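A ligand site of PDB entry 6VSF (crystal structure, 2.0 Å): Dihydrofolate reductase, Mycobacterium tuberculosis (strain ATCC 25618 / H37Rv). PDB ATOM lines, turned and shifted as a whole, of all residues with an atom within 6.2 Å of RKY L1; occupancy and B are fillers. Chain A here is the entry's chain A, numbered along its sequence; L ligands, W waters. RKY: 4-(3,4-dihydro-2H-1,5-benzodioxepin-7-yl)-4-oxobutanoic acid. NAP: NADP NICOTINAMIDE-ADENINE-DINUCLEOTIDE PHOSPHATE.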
ATOM      1  N   ILE A  22     -25.606  18.532 -10.413  1.00  0.00           N
ATOM      2  CA  ILE A  22     -25.733  17.184 -10.979  1.00  0.00           C
ATOM      3  C   ILE A  22     -25.463  16.190  -9.860  1.00  0.00           C
ATOM      4  O   ILE A  22     -24.447  16.320  -9.172  1.00  0.00           O
ATOM      5  CB  ILE A  22     -24.745  16.973 -12.153  1.00  0.00           C
ATOM      6  CG1 ILE A  22     -24.872  18.065 -13.220  1.00  0.00           C
ATOM      7  CG2 ILE A  22     -24.918  15.574 -12.765  1.00  0.00           C
ATOM      8  CD1 ILE A  22     -23.839  17.930 -14.347  1.00  0.00           C
ATOM      9  N   ASP A  29     -16.405  10.918 -17.953  1.00  0.00           N
ATOM     10  CA  ASP A  29     -17.378  11.666 -18.743  1.00  0.00           C
ATOM     11  C   ASP A  29     -16.916  13.101 -18.963  1.00  0.00           C
ATOM     12  O   ASP A  29     -17.120  13.674 -20.054  1.00  0.00           O
ATOM     13  CB  ASP A  29     -18.739  11.628 -18.071  1.00  0.00           C
ATOM     14  CG  ASP A  29     -19.821  12.141 -18.970  1.00  0.00           C
ATOM     15  OD1 ASP A  29     -19.741  11.843 -20.186  1.00  0.00           O
ATOM     16  OD2 ASP A  29     -20.727  12.844 -18.495  1.00  0.00           O
ATOM     17  N   GLN A  30     -16.269  13.697 -17.960  1.00  0.00           N
ATOM     18  CA  GLN A  30     -15.720  15.038 -18.104  1.00  0.00           C
ATOM     19  C   GLN A  30     -14.619  15.094 -19.168  1.00  0.00           C
ATOM     20  O   GLN A  30     -14.556  16.050 -19.949  1.00  0.00           O
ATOM     21  CB  GLN A  30     -15.188  15.523 -16.748  1.00  0.00           C
ATOM     22  CG  GLN A  30     -16.263  15.416 -15.690  1.00  0.00           C
ATOM     23  CD  GLN A  30     -15.989  16.248 -14.460  1.00  0.00           C
ATOM     24  OE1 GLN A  30     -14.973  16.059 -13.789  1.00  0.00           O
ATOM     25  NE2 GLN A  30     -16.907  17.155 -14.141  1.00  0.00           N
ATOM     26  N   ALA A  31     -13.759  14.080 -19.217  1.00  0.00           N
ATOM     27  CA  ALA A  31     -12.755  14.008 -20.288  1.00  0.00           C
ATOM     28  C   ALA A  31     -13.425  13.835 -21.650  1.00  0.00           C
ATOM     29  O   ALA A  31     -13.037  14.478 -22.632  1.00  0.00           O
ATOM     30  CB  ALA A  31     -11.786  12.850 -20.019  1.00  0.00           C
ATOM     31  N   PHE A  33     -16.452  14.804 -22.481  1.00  0.00           N
ATOM     32  CA  PHE A  33     -17.047  16.115 -22.747  1.00  0.00           C
ATOM     33  C   PHE A  33     -16.014  17.088 -23.296  1.00  0.00           C
ATOM     34  O   PHE A  33     -16.238  17.753 -24.324  1.00  0.00           O
ATOM     35  CB  PHE A  33     -17.683  16.642 -21.456  1.00  0.00           C
ATOM     36  CG  PHE A  33     -18.158  18.082 -21.529  1.00  0.00           C
ATOM     37  CD1 PHE A  33     -17.272  19.144 -21.286  1.00  0.00           C
ATOM     38  CD2 PHE A  33     -19.486  18.366 -21.822  1.00  0.00           C
ATOM     39  CE1 PHE A  33     -17.719  20.470 -21.330  1.00  0.00           C
ATOM     40  CE2 PHE A  33     -19.926  19.689 -21.886  1.00  0.00           C
ATOM     41  CZ  PHE A  33     -19.051  20.734 -21.644  1.00  0.00           C
ATOM     42  N   ARG A  34     -14.894  17.211 -22.594  1.00  0.00           N
ATOM     43  CA  ARG A  34     -13.837  18.127 -23.030  1.00  0.00           C
ATOM     44  C   ARG A  34     -13.377  17.800 -24.449  1.00  0.00           C
ATOM     45  O   ARG A  34     -13.233  18.708 -25.275  1.00  0.00           O
ATOM     46  CB  ARG A  34     -12.668  18.075 -22.050  1.00  0.00           C
ATOM     47  CG  ARG A  34     -11.464  18.888 -22.513  1.00  0.00           C
ATOM     48  CD  ARG A  34     -10.326  18.818 -21.493  1.00  0.00           C
ATOM     49  NE  ARG A  34      -9.124  19.492 -21.985  1.00  0.00           N
ATOM     50  CZ  ARG A  34      -8.635  20.614 -21.469  1.00  0.00           C
ATOM     51  NH1 ARG A  34      -9.239  21.206 -20.452  1.00  0.00           N
ATOM     52  NH2 ARG A  34      -7.524  21.145 -21.982  1.00  0.00           N
ATOM     53  N   GLU A  35     -13.160  16.530 -24.746  1.00  0.00           N
ATOM     54  CA  GLU A  35     -12.730  16.123 -26.090  1.00  0.00           C
ATOM     55  C   GLU A  35     -13.737  16.528 -27.169  1.00  0.00           C
ATOM     56  O   GLU A  35     -13.357  17.061 -28.217  1.00  0.00           O
ATOM     57  CB  GLU A  35     -12.505  14.622 -26.133  1.00  0.00           C
ATOM     58  CG  GLU A  35     -12.271  14.022 -27.527  1.00  0.00           C
ATOM     59  CD  GLU A  35     -10.844  14.197 -27.975  1.00  0.00           C
ATOM     60  OE1 GLU A  35     -10.040  14.630 -27.120  1.00  0.00           O
ATOM     61  OE2 GLU A  35     -10.516  13.882 -29.155  1.00  0.00           O
ATOM     62  N   THR A  37     -16.165  18.756 -27.130  1.00  0.00           N
ATOM     63  CA  THR A  37     -16.462  20.181 -27.262  1.00  0.00           C
ATOM     64  C   THR A  37     -15.235  21.031 -27.574  1.00  0.00           C
ATOM     65  O   THR A  37     -15.402  22.154 -28.041  1.00  0.00           O
ATOM     66  CB  THR A  37     -17.120  20.699 -25.973  1.00  0.00           C
ATOM     67  OG1 THR A  37     -16.236  20.512 -24.864  1.00  0.00           O
ATOM     68  CG2 THR A  37     -18.460  19.969 -25.717  1.00  0.00           C
ATOM     69  N   MET A  38     -14.026  20.540 -27.326  1.00  0.00           N
ATOM     70  CA  MET A  38     -12.848  21.399 -27.407  1.00  0.00           C
ATOM     71  C   MET A  38     -12.712  22.008 -28.788  1.00  0.00           C
ATOM     72  O   MET A  38     -12.908  21.330 -29.806  1.00  0.00           O
ATOM     73  CB  MET A  38     -11.574  20.637 -27.065  1.00  0.00           C
ATOM     74  CG  MET A  38     -10.300  21.472 -27.190  1.00  0.00           C
ATOM     75  SD  MET A  38     -10.247  22.874 -26.040  1.00  0.00           S
ATOM     76  CE  MET A  38     -10.498  22.009 -24.477  1.00  0.00           C
ATOM     77  N   THR A  48     -27.063  26.850 -16.234  1.00  0.00           N
ATOM     78  CA  THR A  48     -25.885  25.992 -16.303  1.00  0.00           C
ATOM     79  C   THR A  48     -24.602  26.810 -16.186  1.00  0.00           C
ATOM     80  O   THR A  48     -23.641  26.373 -15.535  1.00  0.00           O
ATOM     81  CB  THR A  48     -25.895  25.162 -17.580  1.00  0.00           C
ATOM     82  OG1 THR A  48     -27.019  24.273 -17.581  1.00  0.00           O
ATOM     83  CG2 THR A  48     -24.617  24.325 -17.685  1.00  0.00           C
ATOM     84  N   SER A  51     -23.960  27.287 -12.698  1.00  0.00           N
ATOM     85  CA  SER A  51     -23.488  26.113 -11.971  1.00  0.00           C
ATOM     86  C   SER A  51     -21.983  25.938 -12.078  1.00  0.00           C
ATOM     87  O   SER A  51     -21.390  25.227 -11.268  1.00  0.00           O
ATOM     88  CB  SER A  51     -24.185  24.837 -12.467  1.00  0.00           C
ATOM     89  OG  SER A  51     -23.667  24.393 -13.707  1.00  0.00           O
ATOM     90  N   LEU A  52     -21.358  26.573 -13.053  1.00  0.00           N
ATOM     91  CA  LEU A  52     -19.924  26.456 -13.198  1.00  0.00           C
ATOM     92  C   LEU A  52     -19.235  27.368 -12.182  1.00  0.00           C
ATOM     93  O   LEU A  52     -19.622  28.529 -12.047  1.00  0.00           O
ATOM     94  CB  LEU A  52     -19.495  26.823 -14.599  1.00  0.00           C
ATOM     95  CG  LEU A  52     -20.094  25.977 -15.714  1.00  0.00           C
ATOM     96  CD1 LEU A  52     -19.792  26.623 -17.078  1.00  0.00           C
ATOM     97  CD2 LEU A  52     -19.546  24.562 -15.630  1.00  0.00           C
ATOM     98  N   VAL A  56     -13.630  28.302 -13.098  1.00  0.00           N
ATOM     99  CA  VAL A  56     -13.662  27.322 -14.180  1.00  0.00           C
ATOM    100  C   VAL A  56     -14.112  27.990 -15.484  1.00  0.00           C
ATOM    101  O   VAL A  56     -13.726  27.563 -16.576  1.00  0.00           O
ATOM    102  CB  VAL A  56     -14.563  26.133 -13.801  1.00  0.00           C
ATOM    103  CG1 VAL A  56     -14.713  25.159 -14.939  1.00  0.00           C
ATOM    104  CG2 VAL A  56     -13.978  25.419 -12.581  1.00  0.00           C
ATOM    105  N   LEU A  59     -15.079  27.855 -20.066  1.00  0.00           N
ATOM    106  CA  LEU A  59     -14.363  26.622 -20.309  1.00  0.00           C
ATOM    107  C   LEU A  59     -13.303  26.892 -21.367  1.00  0.00           C
ATOM    108  O   LEU A  59     -13.595  27.517 -22.392  1.00  0.00           O
ATOM    109  CB  LEU A  59     -15.310  25.513 -20.748  1.00  0.00           C
ATOM    110  CG  LEU A  59     -16.388  25.160 -19.720  1.00  0.00           C
ATOM    111  CD1 LEU A  59     -17.313  24.065 -20.235  1.00  0.00           C
ATOM    112  CD2 LEU A  59     -15.750  24.752 -18.381  1.00  0.00           C
ATOM    113  N   PRO A  60     -12.054  26.461 -21.158  1.00  0.00           N
ATOM    114  CA  PRO A  60     -10.947  26.916 -22.006  1.00  0.00           C
ATOM    115  C   PRO A  60     -11.020  26.382 -23.433  1.00  0.00           C
ATOM    116  O   PRO A  60     -11.439  25.262 -23.689  1.00  0.00           O
ATOM    117  CB  PRO A  60      -9.712  26.362 -21.296  1.00  0.00           C
ATOM    118  CG  PRO A  60     -10.154  25.983 -19.946  1.00  0.00           C
ATOM    119  CD  PRO A  60     -11.610  25.663 -20.012  1.00  0.00           C
ATOM    120  N   ARG A  62     -12.764  27.265 -25.985  1.00  0.00           N
ATOM    121  CA  ARG A  62     -14.083  27.167 -26.578  1.00  0.00           C
ATOM    122  C   ARG A  62     -14.769  28.534 -26.544  1.00  0.00           C
ATOM    123  O   ARG A  62     -14.585  29.318 -25.611  1.00  0.00           O
ATOM    124  CB  ARG A  62     -14.932  26.117 -25.855  1.00  0.00           C
ATOM    125  CG  ARG A  62     -14.585  24.674 -26.230  1.00  0.00           C
ATOM    126  CD  ARG A  62     -14.852  23.696 -25.066  1.00  0.00           C
ATOM    127  NE  ARG A  62     -13.859  23.810 -24.003  1.00  0.00           N
ATOM    128  CZ  ARG A  62     -13.803  23.013 -22.945  1.00  0.00           C
ATOM    129  NH1 ARG A  62     -14.672  22.027 -22.782  1.00  0.00           N
ATOM    130  NH2 ARG A  62     -12.845  23.204 -22.033  1.00  0.00           N
ATOM    131  N   ILE A  96     -24.554  22.307 -24.396  1.00  0.00           N
ATOM    132  CA  ILE A  96     -24.074  21.568 -23.232  1.00  0.00           C
ATOM    133  C   ILE A  96     -25.081  21.602 -22.084  1.00  0.00           C
ATOM    134  O   ILE A  96     -24.773  21.141 -20.985  1.00  0.00           O
ATOM    135  CB  ILE A  96     -22.697  22.061 -22.773  1.00  0.00           C
ATOM    136  CG1 ILE A  96     -22.768  23.514 -22.289  1.00  0.00           C
ATOM    137  CG2 ILE A  96     -21.697  21.912 -23.910  1.00  0.00           C
ATOM    138  CD1 ILE A  96     -21.504  23.979 -21.490  1.00  0.00           C
HETATM  139  C10 RKY L   1     -18.709  18.398 -18.003  1.00  0.00           C
HETATM  140  C13 RKY L   1     -21.954  19.598 -17.118  1.00  0.00           C
HETATM  141  C15 RKY L   1     -21.315  21.634 -18.348  1.00  0.00           C
HETATM  142  C17 RKY L   1     -19.228  20.712 -17.709  1.00  0.00           C
HETATM  143  O01 RKY L   1     -12.336  21.700 -19.883  1.00  0.00           O
HETATM  144  C02 RKY L   1     -13.180  20.788 -19.633  1.00  0.00           C
HETATM  145  O03 RKY L   1     -14.149  20.620 -20.389  1.00  0.00           O
HETATM  146  C04 RKY L   1     -13.013  19.877 -18.405  1.00  0.00           C
HETATM  147  C05 RKY L   1     -14.364  19.216 -17.944  1.00  0.00           C
HETATM  148  C06 RKY L   1     -15.442  20.331 -17.639  1.00  0.00           C
HETATM  149  O07 RKY L   1     -15.091  21.423 -17.387  1.00  0.00           O
HETATM  150  C08 RKY L   1     -16.955  19.988 -17.716  1.00  0.00           C
HETATM  151  C09 RKY L   1     -17.378  18.667 -17.925  1.00  0.00           C
HETATM  152  C11 RKY L   1     -19.648  19.412 -17.897  1.00  0.00           C
HETATM  153  O12 RKY L   1     -21.023  19.056 -18.028  1.00  0.00           O
HETATM  154  C14 RKY L   1     -22.387  21.018 -17.556  1.00  0.00           C
HETATM  155  O16 RKY L   1     -20.174  21.823 -17.587  1.00  0.00           O
HETATM  156  C18 RKY L   1     -17.870  20.998 -17.614  1.00  0.00           C
HETATM  157  PA  NAP L   2     -30.780  25.779 -18.233  1.00  0.00           P
HETATM  158  O1A NAP L   2     -31.438  25.152 -19.421  1.00  0.00           O
HETATM  159  O2A NAP L   2     -29.335  25.480 -17.940  1.00  0.00           O
HETATM  160  O5B NAP L   2     -30.822  27.434 -18.369  1.00  0.00           O
HETATM  161  C5B NAP L   2     -32.190  27.865 -18.245  1.00  0.00           C
HETATM  162  C4B NAP L   2     -32.136  29.387 -18.588  1.00  0.00           C
HETATM  163  O4B NAP L   2     -31.809  29.531 -19.948  1.00  0.00           O
HETATM  164  C3B NAP L   2     -33.469  30.146 -18.373  1.00  0.00           C
HETATM  165  O3B NAP L   2     -33.634  30.456 -17.020  1.00  0.00           O
HETATM  166  C2B NAP L   2     -33.146  31.440 -19.212  1.00  0.00           C
HETATM  167  O2B NAP L   2     -32.181  32.202 -18.698  1.00  0.00           O
HETATM  168  C1B NAP L   2     -32.444  30.748 -20.422  1.00  0.00           C
HETATM  169  N9A NAP L   2     -33.368  30.400 -21.468  1.00  0.00           N
HETATM  170  C8A NAP L   2     -34.183  29.263 -21.587  1.00  0.00           C
HETATM  171  N7A NAP L   2     -34.923  29.265 -22.710  1.00  0.00           N
HETATM  172  C5A NAP L   2     -34.562  30.465 -23.356  1.00  0.00           C
HETATM  173  C6A NAP L   2     -34.990  31.056 -24.567  1.00  0.00           C
HETATM  174  N6A NAP L   2     -35.916  30.424 -25.368  1.00  0.00           N
HETATM  175  N1A NAP L   2     -34.483  32.270 -24.977  1.00  0.00           N
HETATM  176  C2A NAP L   2     -33.557  32.840 -24.142  1.00  0.00           C
HETATM  177  N3A NAP L   2     -33.065  32.400 -22.939  1.00  0.00           N
HETATM  178  C4A NAP L   2     -33.599  31.180 -22.580  1.00  0.00           C
HETATM  179  O3  NAP L   2     -31.772  25.548 -16.923  1.00  0.00           O
HETATM  180  PN  NAP L   2     -32.237  24.058 -16.513  1.00  0.00           P
HETATM  181  O1N NAP L   2     -33.144  23.449 -17.518  1.00  0.00           O
HETATM  182  O2N NAP L   2     -32.688  24.095 -15.074  1.00  0.00           O
HETATM  183  O5D NAP L   2     -30.879  23.012 -16.516  1.00  0.00           O
HETATM  184  C5D NAP L   2     -30.070  23.288 -15.422  1.00  0.00           C
HETATM  185  C4D NAP L   2     -29.752  21.931 -14.770  1.00  0.00           C
HETATM  186  O4D NAP L   2     -29.175  20.998 -15.728  1.00  0.00           O
HETATM  187  C3D NAP L   2     -28.704  22.088 -13.605  1.00  0.00           C
HETATM  188  O3D NAP L   2     -29.079  21.187 -12.617  1.00  0.00           O
HETATM  189  C2D NAP L   2     -27.408  21.612 -14.294  1.00  0.00           C
HETATM  190  O2D NAP L   2     -26.494  21.097 -13.391  1.00  0.00           O
HETATM  191  C1D NAP L   2     -27.973  20.447 -15.141  1.00  0.00           C
HETATM  192  N1N NAP L   2     -27.075  20.088 -16.229  1.00  0.00           N
HETATM  193  C2N NAP L   2     -26.783  18.756 -16.464  1.00  0.00           C
HETATM  194  C3N NAP L   2     -25.953  18.376 -17.472  1.00  0.00           C
HETATM  195  C7N NAP L   2     -25.717  16.934 -17.655  1.00  0.00           C
HETATM  196  O7N NAP L   2     -25.060  16.446 -18.575  1.00  0.00           O
HETATM  197  N7N NAP L   2     -26.222  16.072 -16.739  1.00  0.00           N
HETATM  198  C4N NAP L   2     -25.288  19.372 -18.356  1.00  0.00           C
HETATM  199  C5N NAP L   2     -25.719  20.767 -18.079  1.00  0.00           C
HETATM  200  C6N NAP L   2     -26.551  21.089 -17.086  1.00  0.00           C
HETATM  201  P2B NAP L   2     -32.659  33.705 -17.856  1.00  0.00           P
HETATM  202  O1X NAP L   2     -33.476  33.067 -16.780  1.00  0.00           O
HETATM  203  O2X NAP L   2     -31.288  34.276 -17.460  1.00  0.00           O
HETATM  204  O3X NAP L   2     -33.384  34.337 -19.001  1.00  0.00           O
HETATM  205  O   HOH W   1     -10.638  22.356 -17.942  1.00  0.00           O
HETATM  206  O   HOH W   2     -22.578  16.815 -19.656  1.00  0.00           O
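The backbone NH (N) of Thr 48 lies within hydrogen-bond range of an oxygen (O2A) of NAP L2 (3.2 Å).
The guanidinium group (NH1) of Arg 34 lies within salt-bridge range of an oxygen (O01) of RKY L1 (3.2 Å).
The side-chain hydroxyl (OG1) of Thr 48 is in hydrogen-bond range of an oxygen (O2A) of NAP L2, 2.6 Å away.
The guanidinium group (NH2) of Arg 62 lies within salt-bridge range of an oxygen (O01) of RKY L1 (2.7 Å).
NE of Arg 62 lies within hydrogen-bond range of O of Pro 60 (2.8 Å).
The backbone carbonyl oxygen (O) of Thr 48 is in hydrogen-bond range of the side-chain hydroxyl (OG) of Ser 51 (2.7 Å).
The guanidinium group of Arg 62 sits at hydrogen-bond distance from the side-chain hydroxyl of Thr 37 (3.0 Å).
The side-chain hydroxyl of Thr 37 is in hydrogen-bond range of the backbone carbonyl oxygen of Phe 33 (2.8 Å).
Ile 22 touches RKY L1.
Gln 30 touches RKY L1.
Phe 33 touches RKY L1.
Thr 48 touches RKY L1 (CG2 to C14, 3.99 Å).
Leu 52 touches RKY L1.
Leu 59 touches RKY L1 (CD2 to O07, 3.5 Å).
Ile 96 touches RKY L1 (CD1 to C15, 3.9 Å).
Hydrophobic or aromatic side chains within 4 Å of RKY L1: Ile 22, Phe 33, Leu 52, Leu 59 and Ile 96.
Nine residues have an atom within 4 Å of RKY L1: Ile 22, Gln 30, Phe 33, Arg 34, Thr 48, Leu 52, Leu 59, Arg 62 and Ile 96.
Along chain A the residues within 4 Å of RKY L1 span positions 22 to 96.
The nearest printed residue that does not touch RKY L1 is Pro 60 (4.03 Å).
Water W1 lies within hydrogen-bond range of O01 of RKY L1 (2.7 Å) and NH1 of Arg 34 (3.1 Å).
Water W2 bridges O7N of NAP L2 (2.7 Å) and O12 of RKY L1 (3.2 Å).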
